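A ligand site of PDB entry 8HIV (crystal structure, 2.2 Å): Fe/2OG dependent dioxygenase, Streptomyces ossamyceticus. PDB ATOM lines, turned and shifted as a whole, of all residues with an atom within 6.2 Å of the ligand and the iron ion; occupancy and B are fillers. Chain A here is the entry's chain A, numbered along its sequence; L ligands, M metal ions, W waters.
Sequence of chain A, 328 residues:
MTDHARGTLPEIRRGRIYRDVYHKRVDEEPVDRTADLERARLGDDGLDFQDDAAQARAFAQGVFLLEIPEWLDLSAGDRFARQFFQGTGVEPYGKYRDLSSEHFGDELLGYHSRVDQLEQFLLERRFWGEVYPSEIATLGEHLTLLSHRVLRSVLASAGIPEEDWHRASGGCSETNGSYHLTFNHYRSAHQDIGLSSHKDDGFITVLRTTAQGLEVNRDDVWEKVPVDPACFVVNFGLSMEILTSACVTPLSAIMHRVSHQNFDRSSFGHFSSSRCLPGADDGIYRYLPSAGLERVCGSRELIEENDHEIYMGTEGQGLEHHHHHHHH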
ATOM      1  N   LEU A 118      36.356 -22.584  -0.440  1.00  0.00           N
ATOM      2  CA  LEU A 118      35.024 -22.203  -0.882  1.00  0.00           C
ATOM      3  C   LEU A 118      35.074 -21.075  -1.906  1.00  0.00           C
ATOM      4  O   LEU A 118      35.804 -20.098  -1.750  1.00  0.00           O
ATOM      5  CB  LEU A 118      34.200 -21.755   0.329  1.00  0.00           C
ATOM      6  CG  LEU A 118      32.788 -21.236   0.064  1.00  0.00           C
ATOM      7  CD1 LEU A 118      31.995 -22.348  -0.547  1.00  0.00           C
ATOM      8  CD2 LEU A 118      32.139 -20.762   1.377  1.00  0.00           C
ATOM      9  N   GLN A 120      31.579 -19.019  -3.945  1.00  0.00           N
ATOM     10  CA  GLN A 120      30.160 -18.877  -3.665  1.00  0.00           C
ATOM     11  C   GLN A 120      29.499 -17.952  -4.683  1.00  0.00           C
ATOM     12  O   GLN A 120      30.114 -17.007  -5.175  1.00  0.00           O
ATOM     13  CB  GLN A 120      29.913 -18.251  -2.289  1.00  0.00           C
ATOM     14  CG  GLN A 120      30.042 -19.182  -1.128  1.00  0.00           C
ATOM     15  CD  GLN A 120      29.598 -18.492   0.127  1.00  0.00           C
ATOM     16  OE1 GLN A 120      30.073 -17.406   0.442  1.00  0.00           O
ATOM     17  NE2 GLN A 120      28.664 -19.106   0.852  1.00  0.00           N
ATOM     18  N   THR A 182      22.132 -19.358  -1.633  1.00  0.00           N
ATOM     19  CA  THR A 182      23.590 -19.299  -1.746  1.00  0.00           C
ATOM     20  C   THR A 182      24.098 -20.616  -2.282  1.00  0.00           C
ATOM     21  O   THR A 182      23.735 -21.677  -1.746  1.00  0.00           O
ATOM     22  CB  THR A 182      24.198 -18.994  -0.371  1.00  0.00           C
ATOM     23  OG1 THR A 182      23.786 -17.688   0.024  1.00  0.00           O
ATOM     24  CG2 THR A 182      25.732 -19.048  -0.401  1.00  0.00           C
ATOM     25  N   ASN A 184      27.493 -22.976  -3.252  1.00  0.00           N
ATOM     26  CA  ASN A 184      28.838 -23.210  -2.728  1.00  0.00           C
ATOM     27  C   ASN A 184      29.572 -24.217  -3.595  1.00  0.00           C
ATOM     28  O   ASN A 184      29.024 -25.273  -3.927  1.00  0.00           O
ATOM     29  CB  ASN A 184      28.816 -23.787  -1.310  1.00  0.00           C
ATOM     30  CG  ASN A 184      28.173 -22.864  -0.301  1.00  0.00           C
ATOM     31  OD1 ASN A 184      28.336 -21.649  -0.351  1.00  0.00           O
ATOM     32  ND2 ASN A 184      27.469 -23.451   0.644  1.00  0.00           N
ATOM     33  N   TYR A 186      33.587 -26.068  -3.505  1.00  0.00           N
ATOM     34  CA  TYR A 186      34.860 -26.190  -2.783  1.00  0.00           C
ATOM     35  C   TYR A 186      35.933 -26.592  -3.788  1.00  0.00           C
ATOM     36  O   TYR A 186      35.849 -27.658  -4.397  1.00  0.00           O
ATOM     37  CB  TYR A 186      34.744 -27.194  -1.625  1.00  0.00           C
ATOM     38  CG  TYR A 186      33.709 -26.714  -0.617  1.00  0.00           C
ATOM     39  CD1 TYR A 186      32.350 -26.963  -0.829  1.00  0.00           C
ATOM     40  CD2 TYR A 186      34.090 -25.930   0.478  1.00  0.00           C
ATOM     41  CE1 TYR A 186      31.383 -26.457   0.051  1.00  0.00           C
ATOM     42  CE2 TYR A 186      33.157 -25.439   1.362  1.00  0.00           C
ATOM     43  CZ  TYR A 186      31.797 -25.701   1.152  1.00  0.00           C
ATOM     44  OH  TYR A 186      30.895 -25.176   2.037  1.00  0.00           O
ATOM     45  N   LEU A 195      35.866 -24.794   4.571  1.00  0.00           N
ATOM     46  CA  LEU A 195      35.268 -23.574   5.092  1.00  0.00           C
ATOM     47  C   LEU A 195      35.522 -23.588   6.594  1.00  0.00           C
ATOM     48  O   LEU A 195      35.206 -24.581   7.259  1.00  0.00           O
ATOM     49  CB  LEU A 195      33.762 -23.513   4.783  1.00  0.00           C
ATOM     50  CG  LEU A 195      32.962 -22.339   5.353  1.00  0.00           C
ATOM     51  CD1 LEU A 195      33.552 -20.975   4.925  1.00  0.00           C
ATOM     52  CD2 LEU A 195      31.511 -22.441   4.886  1.00  0.00           C
ATOM     53  N   HIS A 198      32.641 -21.386  11.965  1.00  0.00           N
ATOM     54  CA  HIS A 198      31.845 -20.176  12.053  1.00  0.00           C
ATOM     55  C   HIS A 198      30.477 -20.556  12.597  1.00  0.00           C
ATOM     56  O   HIS A 198      30.085 -21.733  12.619  1.00  0.00           O
ATOM     57  CB  HIS A 198      31.729 -19.475  10.696  1.00  0.00           C
ATOM     58  CG  HIS A 198      30.947 -20.273   9.699  1.00  0.00           C
ATOM     59  ND1 HIS A 198      31.455 -21.372   9.043  1.00  0.00           N
ATOM     60  CD2 HIS A 198      29.645 -20.171   9.317  1.00  0.00           C
ATOM     61  CE1 HIS A 198      30.513 -21.905   8.282  1.00  0.00           C
ATOM     62  NE2 HIS A 198      29.418 -21.198   8.438  1.00  0.00           N
ATOM     63  N   LYS A 199      29.748 -19.550  13.022  1.00  0.00           N
ATOM     64  CA  LYS A 199      28.326 -19.673  13.251  1.00  0.00           C
ATOM     65  C   LYS A 199      27.630 -18.824  12.192  1.00  0.00           C
ATOM     66  O   LYS A 199      28.132 -17.755  11.816  1.00  0.00           O
ATOM     67  CB  LYS A 199      27.959 -19.208  14.660  1.00  0.00           C
ATOM     68  CG  LYS A 199      28.691 -19.958  15.768  1.00  0.00           C
ATOM     69  CD  LYS A 199      28.496 -19.238  17.124  1.00  0.00           C
ATOM     70  CE  LYS A 199      29.083 -20.036  18.293  1.00  0.00           C
ATOM     71  NZ  LYS A 199      29.025 -19.229  19.565  1.00  0.00           N
ATOM     72  N   ASP A 200      26.494 -19.300  11.689  1.00  0.00           N
ATOM     73  CA  ASP A 200      25.749 -18.532  10.693  1.00  0.00           C
ATOM     74  C   ASP A 200      25.157 -17.282  11.325  1.00  0.00           C
ATOM     75  O   ASP A 200      24.854 -17.260  12.520  1.00  0.00           O
ATOM     76  CB  ASP A 200      24.627 -19.383  10.082  1.00  0.00           C
ATOM     77  CG  ASP A 200      25.153 -20.458   9.163  1.00  0.00           C
ATOM     78  OD1 ASP A 200      26.346 -20.341   8.806  1.00  0.00           O
ATOM     79  OD2 ASP A 200      24.423 -21.426   8.828  1.00  0.00           O
ATOM     80  N   THR A 205      18.955 -21.693   8.819  1.00  0.00           N
ATOM     81  CA  THR A 205      19.627 -22.152   7.621  1.00  0.00           C
ATOM     82  C   THR A 205      19.040 -23.485   7.238  1.00  0.00           C
ATOM     83  O   THR A 205      18.921 -24.371   8.076  1.00  0.00           O
ATOM     84  CB  THR A 205      21.133 -22.315   7.859  1.00  0.00           C
ATOM     85  OG1 THR A 205      21.709 -21.055   8.173  1.00  0.00           O
ATOM     86  CG2 THR A 205      21.794 -22.921   6.624  1.00  0.00           C
ATOM     87  N   LEU A 207      20.136 -26.302   4.631  1.00  0.00           N
ATOM     88  CA  LEU A 207      21.312 -26.655   3.852  1.00  0.00           C
ATOM     89  C   LEU A 207      21.051 -27.934   3.045  1.00  0.00           C
ATOM     90  O   LEU A 207      20.608 -28.943   3.602  1.00  0.00           O
ATOM     91  CB  LEU A 207      22.523 -26.846   4.762  1.00  0.00           C
ATOM     92  CG  LEU A 207      23.859 -27.124   4.064  1.00  0.00           C
ATOM     93  CD1 LEU A 207      24.301 -25.906   3.224  1.00  0.00           C
ATOM     94  CD2 LEU A 207      24.923 -27.461   5.096  1.00  0.00           C
ATOM     95  N   ARG A 208      21.335 -27.875   1.759  1.00  0.00           N
ATOM     96  CA  ARG A 208      21.252 -29.030   0.886  1.00  0.00           C
ATOM     97  C   ARG A 208      22.672 -29.465   0.568  1.00  0.00           C
ATOM     98  O   ARG A 208      23.385 -28.802  -0.202  1.00  0.00           O
ATOM     99  CB  ARG A 208      20.471 -28.703  -0.392  1.00  0.00           C
ATOM    100  CG  ARG A 208      19.927 -29.917  -1.159  1.00  0.00           C
ATOM    101  CD  ARG A 208      21.033 -30.694  -1.882  1.00  0.00           C
ATOM    102  NE  ARG A 208      20.564 -31.526  -2.987  1.00  0.00           N
ATOM    103  CZ  ARG A 208      20.007 -32.720  -2.848  1.00  0.00           C
ATOM    104  NH1 ARG A 208      19.839 -33.232  -1.631  1.00  0.00           N
ATOM    105  NH2 ARG A 208      19.628 -33.408  -3.920  1.00  0.00           N
ATOM    106  N   THR A 209      23.092 -30.569   1.153  1.00  0.00           N
ATOM    107  CA  THR A 209      24.413 -31.133   0.935  1.00  0.00           C
ATOM    108  C   THR A 209      24.232 -32.608   0.622  1.00  0.00           C
ATOM    109  O   THR A 209      23.392 -33.276   1.211  1.00  0.00           O
ATOM    110  CB  THR A 209      25.307 -30.958   2.169  1.00  0.00           C
ATOM    111  OG1 THR A 209      26.606 -31.483   1.866  1.00  0.00           O
ATOM    112  CG2 THR A 209      24.735 -31.714   3.370  1.00  0.00           C
ATOM    113  N   GLY A 213      31.728 -33.835   4.413  1.00  0.00           N
ATOM    114  CA  GLY A 213      32.541 -32.643   4.599  1.00  0.00           C
ATOM    115  C   GLY A 213      32.063 -31.750   5.710  1.00  0.00           C
ATOM    116  O   GLY A 213      32.869 -31.062   6.360  1.00  0.00           O
ATOM    117  N   LEU A 214      30.755 -31.682   5.916  1.00  0.00           N
ATOM    118  CA  LEU A 214      30.246 -30.804   6.965  1.00  0.00           C
ATOM    119  C   LEU A 214      30.563 -31.401   8.327  1.00  0.00           C
ATOM    120  O   LEU A 214      30.430 -32.608   8.535  1.00  0.00           O
ATOM    121  CB  LEU A 214      28.751 -30.575   6.785  1.00  0.00           C
ATOM    122  CG  LEU A 214      28.068 -29.652   7.784  1.00  0.00           C
ATOM    123  CD1 LEU A 214      28.567 -28.184   7.732  1.00  0.00           C
ATOM    124  CD2 LEU A 214      26.564 -29.721   7.523  1.00  0.00           C
ATOM    125  N   ASN A 235      19.980 -25.643  10.722  1.00  0.00           N
ATOM    126  CA  ASN A 235      20.582 -25.152  11.948  1.00  0.00           C
ATOM    127  C   ASN A 235      20.192 -23.694  12.123  1.00  0.00           C
ATOM    128  O   ASN A 235      19.589 -23.081  11.246  1.00  0.00           O
ATOM    129  CB  ASN A 235      22.110 -25.309  11.946  1.00  0.00           C
ATOM    130  CG  ASN A 235      22.764 -24.612  10.759  1.00  0.00           C
ATOM    131  OD1 ASN A 235      23.028 -25.243   9.740  1.00  0.00           O
ATOM    132  ND2 ASN A 235      23.053 -23.320  10.894  1.00  0.00           N
ATOM    133  N   HIS A 256      30.211 -24.662  13.049  1.00  0.00           N
ATOM    134  CA  HIS A 256      30.377 -25.727  12.058  1.00  0.00           C
ATOM    135  C   HIS A 256      31.426 -25.300  11.033  1.00  0.00           C
ATOM    136  O   HIS A 256      31.864 -24.149  10.996  1.00  0.00           O
ATOM    137  CB  HIS A 256      29.036 -26.107  11.399  1.00  0.00           C
ATOM    138  CG  HIS A 256      28.331 -24.942  10.784  1.00  0.00           C
ATOM    139  ND1 HIS A 256      27.773 -23.920  11.528  1.00  0.00           N
ATOM    140  CD2 HIS A 256      28.072 -24.632   9.490  1.00  0.00           C
ATOM    141  CE1 HIS A 256      27.231 -23.021  10.723  1.00  0.00           C
ATOM    142  NE2 HIS A 256      27.374 -23.448   9.485  1.00  0.00           N
ATOM    143  N   ARG A 257      31.825 -26.240  10.202  1.00  0.00           N
ATOM    144  CA  ARG A 257      32.900 -26.011   9.255  1.00  0.00           C
ATOM    145  C   ARG A 257      32.809 -27.099   8.202  1.00  0.00           C
ATOM    146  O   ARG A 257      32.042 -28.065   8.352  1.00  0.00           O
ATOM    147  CB  ARG A 257      34.272 -26.042   9.952  1.00  0.00           C
ATOM    148  CG  ARG A 257      34.717 -27.455  10.295  1.00  0.00           C
ATOM    149  CD  ARG A 257      35.904 -27.465  11.260  1.00  0.00           C
ATOM    150  NE  ARG A 257      36.340 -28.820  11.602  1.00  0.00           N
ATOM    151  CZ  ARG A 257      37.269 -29.110  12.511  1.00  0.00           C
ATOM    152  NH1 ARG A 257      37.871 -28.133  13.197  1.00  0.00           N
ATOM    153  NH2 ARG A 257      37.594 -30.382  12.748  1.00  0.00           N
ATOM    154  N   VAL A 258      33.587 -26.942   7.140  1.00  0.00           N
ATOM    155  CA  VAL A 258      33.686 -27.942   6.077  1.00  0.00           C
ATOM    156  C   VAL A 258      35.144 -28.343   6.004  1.00  0.00           C
ATOM    157  O   VAL A 258      36.023 -27.471   5.842  1.00  0.00           O
ATOM    158  CB  VAL A 258      33.216 -27.402   4.711  1.00  0.00           C
ATOM    159  CG1 VAL A 258      33.482 -28.443   3.631  1.00  0.00           C
ATOM    160  CG2 VAL A 258      31.738 -26.983   4.759  1.00  0.00           C
ATOM    161  N   ARG A 265      33.493 -30.483  -4.204  1.00  0.00           N
ATOM    162  CA  ARG A 265      32.249 -30.657  -3.477  1.00  0.00           C
ATOM    163  C   ARG A 265      31.430 -29.419  -3.791  1.00  0.00           C
ATOM    164  O   ARG A 265      31.971 -28.349  -4.050  1.00  0.00           O
ATOM    165  CB  ARG A 265      32.508 -30.821  -1.973  1.00  0.00           C
ATOM    166  CG  ARG A 265      31.286 -30.995  -1.047  1.00  0.00           C
ATOM    167  CD  ARG A 265      31.736 -31.020   0.452  1.00  0.00           C
ATOM    168  NE  ARG A 265      30.613 -31.177   1.385  1.00  0.00           N
ATOM    169  CZ  ARG A 265      29.916 -30.157   1.872  1.00  0.00           C
ATOM    170  NH1 ARG A 265      30.228 -28.916   1.525  1.00  0.00           N
ATOM    171  NH2 ARG A 265      28.923 -30.361   2.730  1.00  0.00           N
ATOM    172  N   SER A 266      30.100 -29.591  -3.864  1.00  0.00           N
ATOM    173  CA  SER A 266      29.235 -28.437  -3.986  1.00  0.00           C
ATOM    174  C   SER A 266      28.025 -28.653  -3.098  1.00  0.00           C
ATOM    175  O   SER A 266      27.758 -29.773  -2.639  1.00  0.00           O
ATOM    176  CB  SER A 266      28.799 -28.162  -5.439  1.00  0.00           C
ATOM    177  OG  SER A 266      28.010 -29.240  -5.914  1.00  0.00           O
ATOM    178  N   SER A 267      27.318 -27.560  -2.850  1.00  0.00           N
ATOM    179  CA  SER A 267      26.150 -27.547  -1.991  1.00  0.00           C
ATOM    180  C   SER A 267      25.430 -26.225  -2.187  1.00  0.00           C
ATOM    181  O   SER A 267      25.929 -25.332  -2.884  1.00  0.00           O
ATOM    182  CB  SER A 267      26.525 -27.744  -0.520  1.00  0.00           C
ATOM    183  OG  SER A 267      27.240 -26.609  -0.029  1.00  0.00           O
ATOM    184  N   PHE A 268      24.260 -26.096  -1.564  1.00  0.00           N
ATOM    185  CA  PHE A 268      23.624 -24.798  -1.550  1.00  0.00           C
ATOM    186  C   PHE A 268      22.732 -24.696  -0.327  1.00  0.00           C
ATOM    187  O   PHE A 268      22.366 -25.709   0.288  1.00  0.00           O
ATOM    188  CB  PHE A 268      22.842 -24.517  -2.846  1.00  0.00           C
ATOM    189  CG  PHE A 268      21.670 -25.433  -3.099  1.00  0.00           C
ATOM    190  CD1 PHE A 268      20.412 -25.110  -2.597  1.00  0.00           C
ATOM    191  CD2 PHE A 268      21.811 -26.584  -3.851  1.00  0.00           C
ATOM    192  CE1 PHE A 268      19.317 -25.941  -2.826  1.00  0.00           C
ATOM    193  CE2 PHE A 268      20.712 -27.420  -4.112  1.00  0.00           C
ATOM    194  CZ  PHE A 268      19.465 -27.094  -3.594  1.00  0.00           C
ATOM    195  N   PHE A 271      19.197 -19.079   3.550  1.00  0.00           N
ATOM    196  CA  PHE A 271      19.510 -18.423   4.809  1.00  0.00           C
ATOM    197  C   PHE A 271      18.459 -17.351   5.073  1.00  0.00           C
ATOM    198  O   PHE A 271      18.166 -16.542   4.193  1.00  0.00           O
ATOM    199  CB  PHE A 271      20.920 -17.799   4.769  1.00  0.00           C
ATOM    200  CG  PHE A 271      22.040 -18.811   4.549  1.00  0.00           C
ATOM    201  CD1 PHE A 271      22.253 -19.373   3.294  1.00  0.00           C
ATOM    202  CD2 PHE A 271      22.863 -19.196   5.595  1.00  0.00           C
ATOM    203  CE1 PHE A 271      23.284 -20.300   3.085  1.00  0.00           C
ATOM    204  CE2 PHE A 271      23.892 -20.119   5.410  1.00  0.00           C
ATOM    205  CZ  PHE A 271      24.105 -20.681   4.155  1.00  0.00           C
HETATM  206  C1  LIG L   1      27.696 -21.848   4.837  1.00  0.00           C
HETATM  207  O1  LIG L   1      27.645 -20.999   5.768  1.00  0.00           O
HETATM  208  O2  LIG L   1      27.578 -21.468   3.635  1.00  0.00           O
HETATM  209  C2  LIG L   1      27.901 -23.272   5.118  1.00  0.00           C
HETATM  210  O3  LIG L   1      27.985 -23.699   6.275  1.00  0.00           O
HETATM  211  C3  LIG L   1      28.025 -24.237   3.964  1.00  0.00           C
HETATM  212  C4  LIG L   1      28.207 -25.671   4.498  1.00  0.00           C
HETATM  213  C5  LIG L   1      28.334 -26.677   3.358  1.00  0.00           C
HETATM  214  O4  LIG L   1      28.033 -27.858   3.585  1.00  0.00           O
HETATM  215  O5  LIG L   1      28.761 -26.308   2.244  1.00  0.00           O
HETATM  216 FE    FE M   1      27.367 -22.081   7.735  1.00  0.00          FE
HETATM  217  O   HOH W   1      27.131 -18.738   3.192  1.00  0.00           O
HETATM  218  O   HOH W   2      25.389 -23.158   7.115  1.00  0.00           O
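Merely in contact with the ligand: Asn 184, Leu 207, Phe 271, Val 258, Leu 195 and Gln 120. Hydrophobic or aromatic side chains within 4 Å of the ligand: Tyr 186, Leu 195, His 198, Leu 207, His 256, Val 258 and Phe 271.
The iron ion is bound by a ring nitrogen (NE2) of His 256 (2.2 Å), an oxygen (O1) of the ligand (2.3 Å), an oxygen (O3) of the ligand (2.3 Å), the side-chain carboxylate (OD1) of Asp 200 (2.3 Å), water W2 (2.3 Å) and a ring nitrogen (NE2) of His 198 (2.3 Å). The iron ion has six donor atoms within binding distance.
OH of Tyr 186 is in hydrogen-bond range of O5 of the ligand. The side-chain hydroxyl (OG) of Ser 267 sits at hydrogen-bond distance from an oxygen (O5) of the ligand. An oxygen (O4) of the ligand lies within salt-bridge range of the guanidinium group (NH2) of Arg 265 (2.8 Å).
The side-chain amide nitrogen of Asn 235 is in hydrogen-bond range of the side-chain carboxylate of Asp 200, 3.1 Å away. The side-chain carboxylate (OD2) of Asp 200 lies within hydrogen-bond range of the side-chain hydroxyl (OG1) of Thr 205 (2.8 Å). N of Tyr 186 sits at hydrogen-bond distance from O of Arg 265 (2.8 Å). O of Ser 267 sits at hydrogen-bond distance from N of Asn 184 (2.9 Å). The side-chain hydroxyl (OG1) of Thr 209 lies within hydrogen-bond range of the guanidinium group (NH2) of Arg 265, at 2.7 Å. OD1 of Asn 184 is in hydrogen-bond range of NE2 of Gln 120 (2.8 Å). O of Leu 195 is in hydrogen-bond range of N of Val 258 (2.9 Å).
Water W1 lies within hydrogen-bond range of O2 of the ligand (2.8 Å) and NE2 of Gln 120 (2.8 Å).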
